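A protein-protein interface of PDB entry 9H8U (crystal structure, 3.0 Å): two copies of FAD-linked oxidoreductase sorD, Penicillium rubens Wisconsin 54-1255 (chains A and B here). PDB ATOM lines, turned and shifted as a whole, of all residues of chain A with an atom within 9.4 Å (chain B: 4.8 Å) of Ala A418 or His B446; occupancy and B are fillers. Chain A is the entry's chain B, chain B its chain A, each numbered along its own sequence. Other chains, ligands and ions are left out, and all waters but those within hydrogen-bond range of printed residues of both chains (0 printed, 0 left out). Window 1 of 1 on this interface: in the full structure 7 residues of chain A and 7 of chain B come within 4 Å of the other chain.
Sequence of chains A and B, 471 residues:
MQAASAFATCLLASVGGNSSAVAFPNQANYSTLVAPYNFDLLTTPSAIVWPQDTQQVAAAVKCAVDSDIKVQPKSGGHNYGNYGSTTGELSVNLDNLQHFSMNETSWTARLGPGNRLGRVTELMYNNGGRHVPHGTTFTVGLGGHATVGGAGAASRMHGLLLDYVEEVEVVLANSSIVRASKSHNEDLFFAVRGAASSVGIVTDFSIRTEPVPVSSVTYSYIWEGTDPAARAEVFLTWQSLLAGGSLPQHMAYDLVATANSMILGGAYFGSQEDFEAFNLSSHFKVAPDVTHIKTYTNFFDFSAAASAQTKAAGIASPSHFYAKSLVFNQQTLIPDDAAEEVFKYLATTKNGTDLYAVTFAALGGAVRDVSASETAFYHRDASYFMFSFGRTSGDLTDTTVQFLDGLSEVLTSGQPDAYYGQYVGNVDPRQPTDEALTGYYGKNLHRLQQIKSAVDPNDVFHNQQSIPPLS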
ATOM      1  N   LEU A 326     -11.643 -10.711  -8.698  1.00  0.00           N
ATOM      2  CA  LEU A 326     -10.886 -11.901  -9.063  1.00  0.00           C
ATOM      3  C   LEU A 326      -9.785 -11.447 -10.013  1.00  0.00           C
ATOM      4  O   LEU A 326     -10.030 -10.598 -10.866  1.00  0.00           O
ATOM      5  CB  LEU A 326     -11.780 -12.967  -9.733  1.00  0.00           C
ATOM      6  CG  LEU A 326     -12.918 -13.642  -8.922  1.00  0.00           C
ATOM      7  CD1 LEU A 326     -13.956 -14.437  -9.746  1.00  0.00           C
ATOM      8  CD2 LEU A 326     -12.316 -14.551  -7.865  1.00  0.00           C
ATOM      9  N   VAL A 327      -8.576 -11.975  -9.856  1.00  0.00           N
ATOM     10  CA  VAL A 327      -7.500 -11.681 -10.801  1.00  0.00           C
ATOM     11  C   VAL A 327      -7.340 -12.886 -11.720  1.00  0.00           C
ATOM     12  O   VAL A 327      -7.658 -14.021 -11.342  1.00  0.00           O
ATOM     13  CB  VAL A 327      -6.146 -11.364 -10.128  1.00  0.00           C
ATOM     14  CG1 VAL A 327      -5.087 -11.004 -11.202  1.00  0.00           C
ATOM     15  CG2 VAL A 327      -6.285 -10.303  -9.066  1.00  0.00           C
ATOM     16  N   PHE A 328      -6.819 -12.645 -12.928  1.00  0.00           N
ATOM     17  CA  PHE A 328      -6.672 -13.669 -13.952  1.00  0.00           C
ATOM     18  C   PHE A 328      -5.394 -13.396 -14.715  1.00  0.00           C
ATOM     19  O   PHE A 328      -4.851 -12.287 -14.684  1.00  0.00           O
ATOM     20  CB  PHE A 328      -7.874 -13.713 -14.909  1.00  0.00           C
ATOM     21  CG  PHE A 328      -9.125 -14.246 -14.281  1.00  0.00           C
ATOM     22  CD1 PHE A 328      -9.877 -13.466 -13.442  1.00  0.00           C
ATOM     23  CD2 PHE A 328      -9.570 -15.523 -14.562  1.00  0.00           C
ATOM     24  CE1 PHE A 328     -11.033 -13.956 -12.846  1.00  0.00           C
ATOM     25  CE2 PHE A 328     -10.737 -16.031 -13.981  1.00  0.00           C
ATOM     26  CZ  PHE A 328     -11.470 -15.242 -13.125  1.00  0.00           C
ATOM     27  N   ASN A 329      -4.955 -14.412 -15.450  1.00  0.00           N
ATOM     28  CA  ASN A 329      -3.574 -14.545 -15.899  1.00  0.00           C
ATOM     29  C   ASN A 329      -3.503 -15.690 -16.911  1.00  0.00           C
ATOM     30  O   ASN A 329      -4.415 -16.529 -16.977  1.00  0.00           O
ATOM     31  CB  ASN A 329      -2.676 -14.807 -14.698  1.00  0.00           C
ATOM     32  CG  ASN A 329      -3.310 -15.790 -13.727  1.00  0.00           C
ATOM     33  OD1 ASN A 329      -3.662 -16.913 -14.101  1.00  0.00           O
ATOM     34  ND2 ASN A 329      -3.514 -15.355 -12.493  1.00  0.00           N
ATOM     35  N   GLN A 331      -2.577 -18.408 -17.120  1.00  0.00           N
ATOM     36  CA  GLN A 331      -2.806 -19.779 -16.663  1.00  0.00           C
ATOM     37  C   GLN A 331      -4.266 -20.070 -16.285  1.00  0.00           C
ATOM     38  O   GLN A 331      -4.703 -21.224 -16.406  1.00  0.00           O
ATOM     39  CB  GLN A 331      -1.887 -20.105 -15.474  1.00  0.00           C
ATOM     40  CG  GLN A 331      -0.426 -20.486 -15.804  1.00  0.00           C
ATOM     41  CD  GLN A 331       0.387 -19.361 -16.433  1.00  0.00           C
ATOM     42  OE1 GLN A 331       0.657 -18.339 -15.801  1.00  0.00           O
ATOM     43  NE2 GLN A 331       0.807 -19.563 -17.676  1.00  0.00           N
ATOM     44  N   THR A 332      -5.041 -19.077 -15.810  1.00  0.00           N
ATOM     45  CA  THR A 332      -6.464 -19.320 -15.554  1.00  0.00           C
ATOM     46  C   THR A 332      -7.370 -18.580 -16.543  1.00  0.00           C
ATOM     47  O   THR A 332      -8.577 -18.484 -16.302  1.00  0.00           O
ATOM     48  CB  THR A 332      -6.860 -18.991 -14.101  1.00  0.00           C
ATOM     49  OG1 THR A 332      -7.021 -17.590 -13.924  1.00  0.00           O
ATOM     50  CG2 THR A 332      -5.815 -19.452 -13.134  1.00  0.00           C
ATOM     51  N   LEU A 333      -6.808 -18.085 -17.656  1.00  0.00           N
ATOM     52  CA  LEU A 333      -7.541 -17.471 -18.768  1.00  0.00           C
ATOM     53  C   LEU A 333      -8.823 -18.252 -19.068  1.00  0.00           C
ATOM     54  O   LEU A 333      -8.737 -19.352 -19.618  1.00  0.00           O
ATOM     55  CB  LEU A 333      -6.629 -17.404 -20.007  1.00  0.00           C
ATOM     56  CG  LEU A 333      -5.509 -16.360 -19.944  1.00  0.00           C
ATOM     57  CD1 LEU A 333      -4.437 -16.441 -21.034  1.00  0.00           C
ATOM     58  CD2 LEU A 333      -6.155 -15.033 -20.001  1.00  0.00           C
ATOM     59  N   THR A 412     -15.071 -19.259 -12.213  1.00  0.00           N
ATOM     60  CA  THR A 412     -13.960 -20.081 -11.802  1.00  0.00           C
ATOM     61  C   THR A 412     -14.071 -21.525 -12.286  1.00  0.00           C
ATOM     62  O   THR A 412     -13.043 -22.214 -12.319  1.00  0.00           O
ATOM     63  CB  THR A 412     -13.853 -19.987 -10.284  1.00  0.00           C
ATOM     64  OG1 THR A 412     -15.029 -20.534  -9.687  1.00  0.00           O
ATOM     65  CG2 THR A 412     -13.789 -18.532  -9.910  1.00  0.00           C
ATOM     66  N   SER A 413     -15.261 -21.989 -12.728  1.00  0.00           N
ATOM     67  CA  SER A 413     -15.432 -23.375 -13.189  1.00  0.00           C
ATOM     68  C   SER A 413     -14.368 -23.791 -14.203  1.00  0.00           C
ATOM     69  O   SER A 413     -14.101 -24.992 -14.336  1.00  0.00           O
ATOM     70  CB  SER A 413     -16.813 -23.618 -13.818  1.00  0.00           C
ATOM     71  OG  SER A 413     -17.304 -22.490 -14.528  1.00  0.00           O
ATOM     72  N   GLY A 414     -13.790 -22.832 -14.937  1.00  0.00           N
ATOM     73  CA  GLY A 414     -12.553 -23.035 -15.677  1.00  0.00           C
ATOM     74  C   GLY A 414     -11.580 -23.987 -15.000  1.00  0.00           C
ATOM     75  O   GLY A 414     -11.423 -25.123 -15.449  1.00  0.00           O
ATOM     76  N   GLN A 415     -10.921 -23.531 -13.926  1.00  0.00           N
ATOM     77  CA  GLN A 415     -10.089 -24.368 -13.053  1.00  0.00           C
ATOM     78  C   GLN A 415     -10.504 -24.116 -11.614  1.00  0.00           C
ATOM     79  O   GLN A 415      -9.797 -23.419 -10.868  1.00  0.00           O
ATOM     80  CB  GLN A 415      -8.611 -24.038 -13.201  1.00  0.00           C
ATOM     81  CG  GLN A 415      -8.063 -24.370 -14.505  1.00  0.00           C
ATOM     82  CD  GLN A 415      -6.946 -23.466 -14.814  1.00  0.00           C
ATOM     83  OE1 GLN A 415      -6.067 -23.279 -13.995  1.00  0.00           O
ATOM     84  NE2 GLN A 415      -6.957 -22.889 -16.002  1.00  0.00           N
ATOM     85  N   PRO A 416     -11.630 -24.690 -11.175  1.00  0.00           N
ATOM     86  CA  PRO A 416     -12.263 -24.224  -9.930  1.00  0.00           C
ATOM     87  C   PRO A 416     -11.334 -24.109  -8.735  1.00  0.00           C
ATOM     88  O   PRO A 416     -11.710 -23.493  -7.734  1.00  0.00           O
ATOM     89  CB  PRO A 416     -13.349 -25.278  -9.667  1.00  0.00           C
ATOM     90  CG  PRO A 416     -12.957 -26.446 -10.440  1.00  0.00           C
ATOM     91  CD  PRO A 416     -12.260 -25.924 -11.670  1.00  0.00           C
ATOM     92  N   ASP A 417     -10.131 -24.682  -8.814  1.00  0.00           N
ATOM     93  CA  ASP A 417      -9.235 -24.737  -7.663  1.00  0.00           C
ATOM     94  C   ASP A 417      -7.916 -23.986  -7.853  1.00  0.00           C
ATOM     95  O   ASP A 417      -7.079 -24.014  -6.947  1.00  0.00           O
ATOM     96  CB  ASP A 417      -8.939 -26.204  -7.272  1.00  0.00           C
ATOM     97  CG  ASP A 417     -10.218 -27.072  -7.092  1.00  0.00           C
ATOM     98  OD1 ASP A 417     -11.050 -26.811  -6.176  1.00  0.00           O
ATOM     99  OD2 ASP A 417     -10.371 -28.037  -7.881  1.00  0.00           O
ATOM    100  N   ALA A 418      -7.698 -23.304  -8.975  1.00  0.00           N
ATOM    101  CA  ALA A 418      -6.444 -22.581  -9.143  1.00  0.00           C
ATOM    102  C   ALA A 418      -6.404 -21.349  -8.215  1.00  0.00           C
ATOM    103  O   ALA A 418      -7.401 -20.994  -7.576  1.00  0.00           O
ATOM    104  CB  ALA A 418      -6.261 -22.202 -10.614  1.00  0.00           C
ATOM    105  N   TYR A 419      -5.226 -20.696  -8.122  1.00  0.00           N
ATOM    106  CA  TYR A 419      -5.081 -19.477  -7.310  1.00  0.00           C
ATOM    107  C   TYR A 419      -5.682 -18.286  -8.044  1.00  0.00           C
ATOM    108  O   TYR A 419      -5.137 -17.811  -9.057  1.00  0.00           O
ATOM    109  CB  TYR A 419      -3.629 -19.169  -6.934  1.00  0.00           C
ATOM    110  CG  TYR A 419      -3.516 -17.853  -6.151  1.00  0.00           C
ATOM    111  CD1 TYR A 419      -4.384 -17.586  -5.093  1.00  0.00           C
ATOM    112  CD2 TYR A 419      -2.570 -16.870  -6.484  1.00  0.00           C
ATOM    113  CE1 TYR A 419      -4.320 -16.392  -4.378  1.00  0.00           C
ATOM    114  CE2 TYR A 419      -2.499 -15.662  -5.764  1.00  0.00           C
ATOM    115  CZ  TYR A 419      -3.384 -15.434  -4.706  1.00  0.00           C
ATOM    116  OH  TYR A 419      -3.359 -14.265  -3.956  1.00  0.00           O
ATOM    117  N   TYR A 420      -6.788 -17.788  -7.492  1.00  0.00           N
ATOM    118  CA  TYR A 420      -7.564 -16.682  -8.038  1.00  0.00           C
ATOM    119  C   TYR A 420      -7.372 -15.503  -7.083  1.00  0.00           C
ATOM    120  O   TYR A 420      -7.842 -15.538  -5.936  1.00  0.00           O
ATOM    121  CB  TYR A 420      -9.040 -17.085  -8.155  1.00  0.00           C
ATOM    122  CG  TYR A 420      -9.429 -17.904  -9.389  1.00  0.00           C
ATOM    123  CD1 TYR A 420      -9.081 -17.489 -10.671  1.00  0.00           C
ATOM    124  CD2 TYR A 420     -10.190 -19.070  -9.272  1.00  0.00           C
ATOM    125  CE1 TYR A 420      -9.454 -18.229 -11.800  1.00  0.00           C
ATOM    126  CE2 TYR A 420     -10.567 -19.810 -10.393  1.00  0.00           C
ATOM    127  CZ  TYR A 420     -10.199 -19.383 -11.657  1.00  0.00           C
ATOM    128  OH  TYR A 420     -10.571 -20.097 -12.785  1.00  0.00           O
ATOM    129  N   GLY A 421      -6.653 -14.475  -7.535  1.00  0.00           N
ATOM    130  CA  GLY A 421      -6.404 -13.313  -6.675  1.00  0.00           C
ATOM    131  C   GLY A 421      -7.605 -12.368  -6.587  1.00  0.00           C
ATOM    132  O   GLY A 421      -8.331 -12.161  -7.558  1.00  0.00           O
ATOM    133  N   LYS B 443       4.096 -23.481  -4.737  1.00  0.00           N
ATOM    134  CA  LYS B 443       2.721 -23.205  -5.116  1.00  0.00           C
ATOM    135  C   LYS B 443       2.335 -23.891  -6.421  1.00  0.00           C
ATOM    136  O   LYS B 443       1.142 -24.152  -6.629  1.00  0.00           O
ATOM    137  CB  LYS B 443       2.478 -21.696  -5.192  1.00  0.00           C
ATOM    138  N   ASN B 444       3.307 -24.223  -7.285  1.00  0.00           N
ATOM    139  CA  ASN B 444       3.011 -25.009  -8.485  1.00  0.00           C
ATOM    140  C   ASN B 444       2.462 -26.398  -8.158  1.00  0.00           C
ATOM    141  O   ASN B 444       1.986 -27.089  -9.061  1.00  0.00           O
ATOM    142  CB  ASN B 444       4.260 -25.180  -9.364  1.00  0.00           C
ATOM    143  CG  ASN B 444       4.647 -23.920 -10.125  1.00  0.00           C
ATOM    144  OD1 ASN B 444       3.839 -23.005 -10.300  1.00  0.00           O
ATOM    145  ND2 ASN B 444       5.913 -23.853 -10.546  1.00  0.00           N
ATOM    146  N   LEU B 445       2.516 -26.827  -6.901  1.00  0.00           N
ATOM    147  CA  LEU B 445       2.134 -28.192  -6.604  1.00  0.00           C
ATOM    148  C   LEU B 445       0.716 -28.472  -7.049  1.00  0.00           C
ATOM    149  O   LEU B 445       0.397 -29.590  -7.455  1.00  0.00           O
ATOM    150  CB  LEU B 445       2.295 -28.469  -5.118  1.00  0.00           C
ATOM    151  CG  LEU B 445       1.676 -29.766  -4.600  1.00  0.00           C
ATOM    152  CD1 LEU B 445       2.150 -30.944  -5.417  1.00  0.00           C
ATOM    153  CD2 LEU B 445       2.058 -29.933  -3.139  1.00  0.00           C
ATOM    154  N   HIS B 446      -0.160 -27.479  -6.973  1.00  0.00           N
ATOM    155  CA  HIS B 446      -1.542 -27.773  -7.308  1.00  0.00           C
ATOM    156  C   HIS B 446      -1.754 -27.849  -8.809  1.00  0.00           C
ATOM    157  O   HIS B 446      -2.374 -28.793  -9.298  1.00  0.00           O
ATOM    158  CB  HIS B 446      -2.489 -26.757  -6.696  1.00  0.00           C
ATOM    159  CG  HIS B 446      -3.895 -26.925  -7.176  1.00  0.00           C
ATOM    160  ND1 HIS B 446      -4.390 -26.240  -8.270  1.00  0.00           N
ATOM    161  CD2 HIS B 446      -4.891 -27.747  -6.761  1.00  0.00           C
ATOM    162  CE1 HIS B 446      -5.644 -26.605  -8.486  1.00  0.00           C
ATOM    163  NE2 HIS B 446      -5.972 -27.520  -7.587  1.00  0.00           N
ATOM    164  N   ARG B 447      -1.246 -26.888  -9.577  1.00  0.00           N
ATOM    165  CA  ARG B 447      -1.335 -27.068 -11.026  1.00  0.00           C
ATOM    166  C   ARG B 447      -0.787 -28.425 -11.441  1.00  0.00           C
ATOM    167  O   ARG B 447      -1.315 -29.069 -12.352  1.00  0.00           O
ATOM    168  CB  ARG B 447      -0.595 -25.958 -11.776  1.00  0.00           C
ATOM    169  CG  ARG B 447      -0.561 -26.225 -13.260  1.00  0.00           C
ATOM    170  CD  ARG B 447      -0.113 -25.045 -14.068  1.00  0.00           C
ATOM    171  NE  ARG B 447      -0.298 -25.302 -15.497  1.00  0.00           N
ATOM    172  CZ  ARG B 447       0.236 -24.583 -16.481  1.00  0.00           C
ATOM    173  NH1 ARG B 447       1.016 -23.526 -16.237  1.00  0.00           N
ATOM    174  NH2 ARG B 447      -0.039 -24.917 -17.743  1.00  0.00           N
ATOM    175  N   LEU B 448       0.266 -28.888 -10.755  1.00  0.00           N
ATOM    176  CA  LEU B 448       0.876 -30.181 -11.061  1.00  0.00           C
ATOM    177  C   LEU B 448      -0.076 -31.343 -10.752  1.00  0.00           C
ATOM    178  O   LEU B 448      -0.122 -32.335 -11.489  1.00  0.00           O
ATOM    179  CB  LEU B 448       2.195 -30.325 -10.296  1.00  0.00           C
ATOM    180  CG  LEU B 448       3.313 -29.372 -10.744  1.00  0.00           C
ATOM    181  CD1 LEU B 448       4.433 -29.266  -9.717  1.00  0.00           C
ATOM    182  CD2 LEU B 448       3.869 -29.801 -12.079  1.00  0.00           C
ATOM    183  N   GLN B 449      -0.860 -31.252  -9.681  1.00  0.00           N
ATOM    184  CA  GLN B 449      -1.885 -32.270  -9.503  1.00  0.00           C
ATOM    185  C   GLN B 449      -2.929 -32.180 -10.616  1.00  0.00           C
ATOM    186  O   GLN B 449      -3.470 -33.204 -11.047  1.00  0.00           O
ATOM    187  CB  GLN B 449      -2.511 -32.145  -8.125  1.00  0.00           C
ATOM    188  CG  GLN B 449      -1.454 -32.204  -7.072  1.00  0.00           C
ATOM    189  CD  GLN B 449      -2.006 -32.241  -5.675  1.00  0.00           C
ATOM    190  OE1 GLN B 449      -1.756 -31.330  -4.874  1.00  0.00           O
ATOM    191  NE2 GLN B 449      -2.761 -33.296  -5.363  1.00  0.00           N
ATOM    192  N   GLN B 450      -3.209 -30.969 -11.116  1.00  0.00           N
ATOM    193  CA  GLN B 450      -4.129 -30.847 -12.241  1.00  0.00           C
ATOM    194  C   GLN B 450      -3.608 -31.608 -13.451  1.00  0.00           C
ATOM    195  O   GLN B 450      -4.340 -32.377 -14.080  1.00  0.00           O
ATOM    196  CB  GLN B 450      -4.392 -29.382 -12.604  1.00  0.00           C
ATOM    197  CG  GLN B 450      -5.464 -28.688 -11.754  1.00  0.00           C
ATOM    198  CD  GLN B 450      -5.808 -27.271 -12.250  1.00  0.00           C
ATOM    199  OE1 GLN B 450      -5.313 -26.823 -13.288  1.00  0.00           O
ATOM    200  NE2 GLN B 450      -6.680 -26.579 -11.514  1.00  0.00           N
ATOM    201  N   LEU B 470      -5.366 -35.649  -8.187  1.00  0.00           N
ATOM    202  CA  LEU B 470      -6.350 -34.961  -7.360  1.00  0.00           C
ATOM    203  C   LEU B 470      -7.388 -35.922  -6.763  1.00  0.00           C
ATOM    204  O   LEU B 470      -7.532 -37.085  -7.170  1.00  0.00           O
ATOM    205  CB  LEU B 470      -7.050 -33.867  -8.175  1.00  0.00           C
ATOM    206  CG  LEU B 470      -6.141 -32.674  -8.485  1.00  0.00           C
ATOM    207  CD1 LEU B 470      -6.708 -31.689  -9.494  1.00  0.00           C
ATOM    208  CD2 LEU B 470      -5.841 -31.944  -7.188  1.00  0.00           C
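O of Gln A331 is in hydrogen-bond range of NE2 of Gln A415 (2.8 Å).
Arg B447 touches Gln A331 (NH1 to CG, 3.4 Å). Gln A415 touches Gln B450. His B446 touches Asp A417 (NE2 to CB, 3.3 Å). CE1 of His B446 touches N of Ala A418 (3.9 Å).
Ala A418 touches just one residue of chain B: His B446. Of the printed residues of chain A, His B446 touches Asp A417 (3.3 Å) and Ala A418 (3.9 Å). No residue of chain A comes within 4 Å of Leu B445. Of the printed residues of chain A, Gln B450 touches Gln A415. Of the printed residues of chain B, Asp A417 touches His B446 (3.3 Å). Printed residues of chain B within 4 Å of Gln A331: Arg B447. Printed residues of chain A within 4 Å of Arg B447: Gln A331. The nearest residue of chain A that does not touch His B446 is Tyr A419 (5.6 Å).
Of the 17 printed residues of chain A, 4 touch a printed residue of chain B. Hydrophobic or aromatic side chains of chain B that line the printed part of chain A: His B446. Among the printed residues, 4 pairs touch across the chains. Among the printed residues, no Asp or Glu carboxylate lies within 4 Å of a Lys or Arg side-chain nitrogen of the other chain.
No position is printed for both chains.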
